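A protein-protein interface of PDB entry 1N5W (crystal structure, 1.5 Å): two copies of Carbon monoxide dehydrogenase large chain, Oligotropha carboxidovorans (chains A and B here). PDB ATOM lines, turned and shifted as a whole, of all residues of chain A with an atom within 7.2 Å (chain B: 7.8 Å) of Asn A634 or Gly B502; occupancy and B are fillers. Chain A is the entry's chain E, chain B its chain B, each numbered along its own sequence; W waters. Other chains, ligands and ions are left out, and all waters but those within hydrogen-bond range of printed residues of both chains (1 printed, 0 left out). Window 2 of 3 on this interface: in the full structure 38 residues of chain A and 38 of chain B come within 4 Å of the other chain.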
ATOM      1  N   PRO A 515      15.270   7.292   6.984  1.00  0.00           N
ATOM      2  CA  PRO A 515      14.583   8.575   6.818  1.00  0.00           C
ATOM      3  C   PRO A 515      14.208   8.903   5.404  1.00  0.00           C
ATOM      4  O   PRO A 515      13.137   9.521   5.174  1.00  0.00           O
ATOM      5  CB  PRO A 515      15.560   9.588   7.389  1.00  0.00           C
ATOM      6  CG  PRO A 515      16.408   8.789   8.420  1.00  0.00           C
ATOM      7  CD  PRO A 515      16.479   7.414   7.832  1.00  0.00           C
ATOM      8  N   MET A 598      -0.939  13.701  10.609  1.00  0.00           N
ATOM      9  CA  MET A 598      -0.536  14.725   9.637  1.00  0.00           C
ATOM     10  C   MET A 598      -1.767  15.385   9.005  1.00  0.00           C
ATOM     11  O   MET A 598      -1.765  16.604   8.719  1.00  0.00           O
ATOM     12  CB  MET A 598       0.375  14.140   8.537  1.00  0.00           C
ATOM     13  CG  MET A 598       1.727  13.688   9.067  1.00  0.00           C
ATOM     14  SD  MET A 598       2.819  13.133   7.756  1.00  0.00           S
ATOM     15  CE  MET A 598       3.604  14.662   7.300  1.00  0.00           C
ATOM     16  N   GLU A 627       6.732   9.920   2.280  1.00  0.00           N
ATOM     17  CA  GLU A 627       6.532  11.087   3.136  1.00  0.00           C
ATOM     18  C   GLU A 627       6.320  10.703   4.578  1.00  0.00           C
ATOM     19  O   GLU A 627       6.803  11.412   5.459  1.00  0.00           O
ATOM     20  CB  GLU A 627       5.294  11.899   2.673  1.00  0.00           C
ATOM     21  CG  GLU A 627       5.348  12.418   1.274  1.00  0.00           C
ATOM     22  CD  GLU A 627       4.037  13.123   0.886  1.00  0.00           C
ATOM     23  OE1 GLU A 627       4.122  14.317   0.550  1.00  0.00           O
ATOM     24  OE2 GLU A 627       2.938  12.521   0.945  1.00  0.00           O
ATOM     25  N   LEU A 628       5.665   9.581   4.827  1.00  0.00           N
ATOM     26  CA  LEU A 628       5.394   9.100   6.175  1.00  0.00           C
ATOM     27  C   LEU A 628       6.678   8.626   6.848  1.00  0.00           C
ATOM     28  O   LEU A 628       6.887   8.843   8.041  1.00  0.00           O
ATOM     29  CB  LEU A 628       4.307   8.010   6.168  1.00  0.00           C
ATOM     30  CG  LEU A 628       2.938   8.482   5.697  1.00  0.00           C
ATOM     31  CD1 LEU A 628       2.024   7.334   5.356  1.00  0.00           C
ATOM     32  CD2 LEU A 628       2.327   9.390   6.726  1.00  0.00           C
ATOM     33  N   ALA A 629       7.531   7.911   6.119  1.00  0.00           N
ATOM     34  CA  ALA A 629       8.846   7.517   6.610  1.00  0.00           C
ATOM     35  C   ALA A 629       9.648   8.758   7.032  1.00  0.00           C
ATOM     36  O   ALA A 629      10.254   8.797   8.099  1.00  0.00           O
ATOM     37  CB  ALA A 629       9.620   6.740   5.547  1.00  0.00           C
ATOM     38  N   TRP A 630       9.696   9.796   6.209  1.00  0.00           N
ATOM     39  CA  TRP A 630      10.380  11.021   6.600  1.00  0.00           C
ATOM     40  C   TRP A 630       9.743  11.665   7.814  1.00  0.00           C
ATOM     41  O   TRP A 630      10.452  12.014   8.771  1.00  0.00           O
ATOM     42  CB  TRP A 630      10.461  12.048   5.447  1.00  0.00           C
ATOM     43  CG  TRP A 630      11.065  13.349   5.789  1.00  0.00           C
ATOM     44  CD1 TRP A 630      10.397  14.565   5.818  1.00  0.00           C
ATOM     45  CD2 TRP A 630      12.369  13.616   6.312  1.00  0.00           C
ATOM     46  NE1 TRP A 630      11.246  15.567   6.226  1.00  0.00           N
ATOM     47  CE2 TRP A 630      12.482  15.021   6.454  1.00  0.00           C
ATOM     48  CE3 TRP A 630      13.497  12.852   6.543  1.00  0.00           C
ATOM     49  CZ2 TRP A 630      13.631  15.628   6.936  1.00  0.00           C
ATOM     50  CZ3 TRP A 630      14.654  13.464   6.937  1.00  0.00           C
ATOM     51  CH2 TRP A 630      14.701  14.842   7.180  1.00  0.00           C
ATOM     52  N   ALA A 631       8.420  11.721   7.854  1.00  0.00           N
ATOM     53  CA  ALA A 631       7.752  12.281   9.002  1.00  0.00           C
ATOM     54  C   ALA A 631       8.049  11.540  10.308  1.00  0.00           C
ATOM     55  O   ALA A 631       8.135  12.137  11.365  1.00  0.00           O
ATOM     56  CB  ALA A 631       6.256  12.320   8.795  1.00  0.00           C
ATOM     57  N   SER A 632       8.244  10.249  10.240  1.00  0.00           N
ATOM     58  CA  SER A 632       8.511   9.495  11.433  1.00  0.00           C
ATOM     59  C   SER A 632       9.805   9.916  12.106  1.00  0.00           C
ATOM     60  O   SER A 632       9.953   9.686  13.328  1.00  0.00           O
ATOM     61  CB  SER A 632       8.530   8.000  11.116  1.00  0.00           C
ATOM     62  OG  SER A 632       9.789   7.538  10.624  1.00  0.00           O
ATOM     63  N   TYR A 633      10.721  10.527  11.359  1.00  0.00           N
ATOM     64  CA  TYR A 633      11.996  11.032  11.888  1.00  0.00           C
ATOM     65  C   TYR A 633      11.972  12.560  12.111  1.00  0.00           C
ATOM     66  O   TYR A 633      12.574  13.040  13.045  1.00  0.00           O
ATOM     67  CB  TYR A 633      13.152  10.670  10.943  1.00  0.00           C
ATOM     68  CG  TYR A 633      13.531   9.207  10.837  1.00  0.00           C
ATOM     69  CD1 TYR A 633      12.897   8.359   9.976  1.00  0.00           C
ATOM     70  CD2 TYR A 633      14.507   8.643  11.657  1.00  0.00           C
ATOM     71  CE1 TYR A 633      13.258   7.021   9.868  1.00  0.00           C
ATOM     72  CE2 TYR A 633      14.852   7.292  11.574  1.00  0.00           C
ATOM     73  CZ  TYR A 633      14.237   6.479  10.667  1.00  0.00           C
ATOM     74  OH  TYR A 633      14.612   5.172  10.515  1.00  0.00           O
ATOM     75  N   ASN A 634      11.296  13.285  11.213  1.00  0.00           N
ATOM     76  CA  ASN A 634      11.319  14.756  11.122  1.00  0.00           C
ATOM     77  C   ASN A 634      10.208  15.379  11.999  1.00  0.00           C
ATOM     78  O   ASN A 634      10.404  16.414  12.592  1.00  0.00           O
ATOM     79  CB  ASN A 634      11.113  15.146   9.648  1.00  0.00           C
ATOM     80  CG  ASN A 634      10.709  16.596   9.431  1.00  0.00           C
ATOM     81  OD1 ASN A 634       9.503  16.917   9.208  1.00  0.00           O
ATOM     82  ND2 ASN A 634      11.678  17.525   9.563  1.00  0.00           N
ATOM     83  N   SER A 635       9.042  14.758  12.036  1.00  0.00           N
ATOM     84  CA  SER A 635       7.898  15.276  12.775  1.00  0.00           C
ATOM     85  C   SER A 635       7.110  14.175  13.455  1.00  0.00           C
ATOM     86  O   SER A 635       5.940  13.927  13.129  1.00  0.00           O
ATOM     87  CB  SER A 635       6.979  16.060  11.862  1.00  0.00           C
ATOM     88  OG  SER A 635       7.652  17.105  11.202  1.00  0.00           O
ATOM     89  N   PRO A 636       7.787  13.425  14.319  1.00  0.00           N
ATOM     90  CA  PRO A 636       7.145  12.261  14.904  1.00  0.00           C
ATOM     91  C   PRO A 636       5.924  12.698  15.704  1.00  0.00           C
ATOM     92  O   PRO A 636       5.994  13.665  16.489  1.00  0.00           O
ATOM     93  CB  PRO A 636       8.264  11.636  15.761  1.00  0.00           C
ATOM     94  CG  PRO A 636       9.163  12.773  16.074  1.00  0.00           C
ATOM     95  CD  PRO A 636       9.136  13.636  14.830  1.00  0.00           C
ATOM     96  N   PRO A 642       9.437   7.943  17.625  1.00  0.00           N
ATOM     97  CA  PRO A 642      10.029   8.167  16.320  1.00  0.00           C
ATOM     98  C   PRO A 642      10.418   6.897  15.561  1.00  0.00           C
ATOM     99  O   PRO A 642      10.522   5.829  16.168  1.00  0.00           O
ATOM    100  CB  PRO A 642      11.236   9.032  16.625  1.00  0.00           C
ATOM    101  CG  PRO A 642      10.913   9.673  17.916  1.00  0.00           C
ATOM    102  CD  PRO A 642      10.183   8.613  18.708  1.00  0.00           C
ATOM    103  N   GLY A 643      10.762   7.079  14.294  1.00  0.00           N
ATOM    104  CA  GLY A 643      11.214   5.971  13.451  1.00  0.00           C
ATOM    105  C   GLY A 643      10.069   5.128  12.892  1.00  0.00           C
ATOM    106  O   GLY A 643       8.903   5.369  13.178  1.00  0.00           O
ATOM    107  N   PRO B 348      21.767  22.157  16.977  1.00  0.00           N
ATOM    108  CA  PRO B 348      20.387  21.956  16.502  1.00  0.00           C
ATOM    109  C   PRO B 348      20.055  23.065  15.487  1.00  0.00           C
ATOM    110  O   PRO B 348      20.445  24.223  15.723  1.00  0.00           O
ATOM    111  CB  PRO B 348      19.597  22.022  17.801  1.00  0.00           C
ATOM    112  CG  PRO B 348      20.560  21.773  18.894  1.00  0.00           C
ATOM    113  CD  PRO B 348      21.843  22.417  18.428  1.00  0.00           C
ATOM    114  N   SER B 349      19.267  22.788  14.458  1.00  0.00           N
ATOM    115  CA  SER B 349      19.075  23.705  13.342  1.00  0.00           C
ATOM    116  C   SER B 349      18.428  25.019  13.724  1.00  0.00           C
ATOM    117  O   SER B 349      18.592  26.018  13.012  1.00  0.00           O
ATOM    118  CB  SER B 349      18.299  23.063  12.190  1.00  0.00           C
ATOM    119  OG  SER B 349      16.913  23.111  12.433  1.00  0.00           O
ATOM    120  N   LYS B 350      17.634  25.074  14.779  1.00  0.00           N
ATOM    121  CA  LYS B 350      16.930  26.277  15.171  1.00  0.00           C
ATOM    122  C   LYS B 350      17.704  27.153  16.181  1.00  0.00           C
ATOM    123  O   LYS B 350      17.186  28.174  16.680  1.00  0.00           O
ATOM    124  CB  LYS B 350      15.554  25.883  15.764  1.00  0.00           C
ATOM    125  CG  LYS B 350      14.601  25.269  14.732  1.00  0.00           C
ATOM    126  CD  LYS B 350      13.321  24.777  15.365  1.00  0.00           C
ATOM    127  CE  LYS B 350      12.444  24.085  14.377  1.00  0.00           C
ATOM    128  NZ  LYS B 350      11.246  23.451  15.001  1.00  0.00           N
ATOM    129  N   SER B 495      11.437  16.893  20.432  1.00  0.00           N
ATOM    130  CA  SER B 495      11.109  17.039  19.019  1.00  0.00           C
ATOM    131  C   SER B 495      10.494  18.418  18.694  1.00  0.00           C
ATOM    132  O   SER B 495      10.666  18.890  17.579  1.00  0.00           O
ATOM    133  CB  SER B 495      10.225  15.893  18.535  1.00  0.00           C
ATOM    134  OG  SER B 495       9.034  15.846  19.288  1.00  0.00           O
ATOM    135  N   LYS B 496       9.905  19.104  19.655  1.00  0.00           N
ATOM    136  CA  LYS B 496       9.319  20.408  19.364  1.00  0.00           C
ATOM    137  C   LYS B 496      10.353  21.321  18.724  1.00  0.00           C
ATOM    138  O   LYS B 496      10.040  22.091  17.821  1.00  0.00           O
ATOM    139  CB  LYS B 496       8.726  21.050  20.620  1.00  0.00           C
ATOM    140  CG  LYS B 496       8.315  22.504  20.459  1.00  0.00           C
ATOM    141  CD  LYS B 496       8.090  23.122  21.845  1.00  0.00           C
ATOM    142  N   CYS B 498      14.223  20.624  18.752  1.00  0.00           N
ATOM    143  CA  CYS B 498      15.596  20.121  18.576  1.00  0.00           C
ATOM    144  C   CYS B 498      15.668  19.151  17.403  1.00  0.00           C
ATOM    145  O   CYS B 498      15.025  18.105  17.423  1.00  0.00           O
ATOM    146  CB  CYS B 498      16.118  19.418  19.844  1.00  0.00           C
ATOM    147  SG  CYS B 498      16.334  20.595  21.229  1.00  0.00           S
ATOM    148  N   ASP B 499      16.438  19.514  16.380  1.00  0.00           N
ATOM    149  CA  ASP B 499      16.606  18.674  15.225  1.00  0.00           C
ATOM    150  C   ASP B 499      17.981  18.918  14.628  1.00  0.00           C
ATOM    151  O   ASP B 499      18.497  20.048  14.733  1.00  0.00           O
ATOM    152  CB  ASP B 499      15.542  18.940  14.148  1.00  0.00           C
ATOM    153  CG  ASP B 499      15.640  20.334  13.542  1.00  0.00           C
ATOM    154  OD1 ASP B 499      15.047  21.311  14.107  1.00  0.00           O
ATOM    155  OD2 ASP B 499      16.248  20.463  12.490  1.00  0.00           O
ATOM    156  N   ILE B 500      18.543  17.906  13.968  1.00  0.00           N
ATOM    157  CA  ILE B 500      19.766  18.060  13.174  1.00  0.00           C
ATOM    158  C   ILE B 500      19.402  17.948  11.725  1.00  0.00           C
ATOM    159  O   ILE B 500      18.983  16.881  11.281  1.00  0.00           O
ATOM    160  CB  ILE B 500      20.826  17.028  13.567  1.00  0.00           C
ATOM    161  CG1 ILE B 500      21.277  17.193  15.032  1.00  0.00           C
ATOM    162  CG2 ILE B 500      22.001  17.100  12.613  1.00  0.00           C
ATOM    163  CD1 ILE B 500      22.207  18.336  15.293  1.00  0.00           C
ATOM    164  N   LEU B 501      19.489  19.076  11.024  1.00  0.00           N
ATOM    165  CA  LEU B 501      19.051  19.197   9.658  1.00  0.00           C
ATOM    166  C   LEU B 501      17.715  18.462   9.361  1.00  0.00           C
ATOM    167  O   LEU B 501      17.581  17.734   8.371  1.00  0.00           O
ATOM    168  CB  LEU B 501      20.144  18.696   8.728  1.00  0.00           C
ATOM    169  CG  LEU B 501      21.432  19.508   8.796  1.00  0.00           C
ATOM    170  CD1 LEU B 501      22.376  18.982   7.769  1.00  0.00           C
ATOM    171  CD2 LEU B 501      21.239  20.990   8.616  1.00  0.00           C
ATOM    172  N   GLY B 502      16.745  18.649  10.240  1.00  0.00           N
ATOM    173  CA  GLY B 502      15.409  18.130  10.038  1.00  0.00           C
ATOM    174  C   GLY B 502      15.108  16.796  10.706  1.00  0.00           C
ATOM    175  O   GLY B 502      13.979  16.342  10.651  1.00  0.00           O
ATOM    176  N   VAL B 503      16.136  16.143  11.255  1.00  0.00           N
ATOM    177  CA  VAL B 503      15.906  14.886  11.968  1.00  0.00           C
ATOM    178  C   VAL B 503      15.798  15.200  13.445  1.00  0.00           C
ATOM    179  O   VAL B 503      16.728  15.745  14.055  1.00  0.00           O
ATOM    180  CB  VAL B 503      16.967  13.822  11.673  1.00  0.00           C
ATOM    181  CG1 VAL B 503      16.670  12.548  12.479  1.00  0.00           C
ATOM    182  CG2 VAL B 503      17.074  13.510  10.167  1.00  0.00           C
ATOM    183  N   SER B 504      14.644  14.870  14.052  1.00  0.00           N
ATOM    184  CA  SER B 504      14.391  15.158  15.475  1.00  0.00           C
ATOM    185  C   SER B 504      15.495  14.496  16.314  1.00  0.00           C
ATOM    186  O   SER B 504      15.896  13.376  16.011  1.00  0.00           O
ATOM    187  CB  SER B 504      12.996  14.719  15.922  1.00  0.00           C
ATOM    188  OG  SER B 504      12.044  15.140  14.998  1.00  0.00           O
ATOM    189  N   MET B 505      15.842  15.137  17.439  1.00  0.00           N
ATOM    190  CA  MET B 505      16.954  14.665  18.250  1.00  0.00           C
ATOM    191  C   MET B 505      16.613  13.622  19.303  1.00  0.00           C
ATOM    192  O   MET B 505      16.780  13.843  20.514  1.00  0.00           O
ATOM    193  CB  MET B 505      17.717  15.872  18.794  1.00  0.00           C
ATOM    194  CG  MET B 505      18.430  16.651  17.702  1.00  0.00           C
ATOM    195  SD  MET B 505      19.342  18.116  18.234  1.00  0.00           S
ATOM    196  CE  MET B 505      20.854  17.268  18.879  1.00  0.00           C
ATOM    197  N   PHE B 506      15.957  12.566  18.861  1.00  0.00           N
ATOM    198  CA  PHE B 506      15.721  11.387  19.702  1.00  0.00           C
ATOM    199  C   PHE B 506      16.965  10.515  19.791  1.00  0.00           C
ATOM    200  O   PHE B 506      17.973  10.804  19.150  1.00  0.00           O
ATOM    201  CB  PHE B 506      14.560  10.583  19.117  1.00  0.00           C
ATOM    202  CG  PHE B 506      14.847  10.045  17.738  1.00  0.00           C
ATOM    203  CD1 PHE B 506      15.524   8.834  17.523  1.00  0.00           C
ATOM    204  CD2 PHE B 506      14.492  10.776  16.633  1.00  0.00           C
ATOM    205  CE1 PHE B 506      15.893   8.428  16.232  1.00  0.00           C
ATOM    206  CE2 PHE B 506      14.730  10.302  15.339  1.00  0.00           C
ATOM    207  CZ  PHE B 506      15.530   9.198  15.153  1.00  0.00           C
ATOM    208  N   LEU B 565      21.124   9.899  16.773  1.00  0.00           N
ATOM    209  CA  LEU B 565      21.632  11.191  16.427  1.00  0.00           C
ATOM    210  C   LEU B 565      23.089  11.387  16.840  1.00  0.00           C
ATOM    211  O   LEU B 565      23.709  12.410  16.552  1.00  0.00           O
ATOM    212  CB  LEU B 565      20.726  12.292  16.942  1.00  0.00           C
ATOM    213  CG  LEU B 565      19.509  12.620  16.058  1.00  0.00           C
ATOM    214  CD1 LEU B 565      19.957  13.277  14.768  1.00  0.00           C
ATOM    215  CD2 LEU B 565      18.639  11.435  15.752  1.00  0.00           C
HETATM  216  O   HOH W   1       8.791  17.789  15.303  1.00  0.00           O
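The backbone carbonyl oxygen of Tyr A633 lies within hydrogen-bond range of the side-chain hydroxyl of Ser B504. O of Gly B502 is in hydrogen-bond range of ND2 of Asn A634, 2.8 Å away. OG of Ser B504 sits at hydrogen-bond distance from O of Asn A634.
N of Gly B502 lies within hydrogen-bond range of OD2 of Asp B499, 2.9 Å away. OG of Ser A635 sits at hydrogen-bond distance from OD1 of Asn A634.
Among the printed residues, pairs that only touch across the chains: Pro A636 with Ser B504, Tyr A633 with Phe B506, Pro A642 with Phe B506, Trp A630 with Gly B502 and Tyr A633 with Val B503.
Asn A634 touches just these residues of chain B: Gly B502 and Ser B504. Of the printed residues of chain B, Tyr A633 touches Val B503, Ser B504 and Phe B506. Printed residues of chain B within 4 Å of Trp A630: Gly B502 (3.8 Å). Of the printed residues of chain B, Pro A636 touches Ser B504 (3.3 Å).
Printed residues of chain A that touch a printed residue of chain B: Trp A630, Tyr A633, Asn A634, Pro A636 and Pro A642. Hydrophobic or aromatic side chains of chain A that line the printed part of chain B: Trp A630, Tyr A633, Pro A636 and Pro A642. Of the 15 printed residues of chain B, 4 touch a printed residue of chain A. Printed residues of chain B that touch a printed residue of chain A: Gly B502, Val B503, Ser B504 and Phe B506. Among the printed residues, 8 pairs touch across the chains. Among the printed residues, no Asp or Glu carboxylate lies within 4 Å of a Lys or Arg side-chain nitrogen of the other chain.
No position is printed for both chains. Of the 8 pairs that touch across the chains among the printed residues, none has its exchanged pair printed and touching as well.
Water W1 bridges the backbone carbonyl oxygen (O) of Ser B495 (3.1 Å) and the backbone carbonyl oxygen (O) of Asn A634 (3.4 Å).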
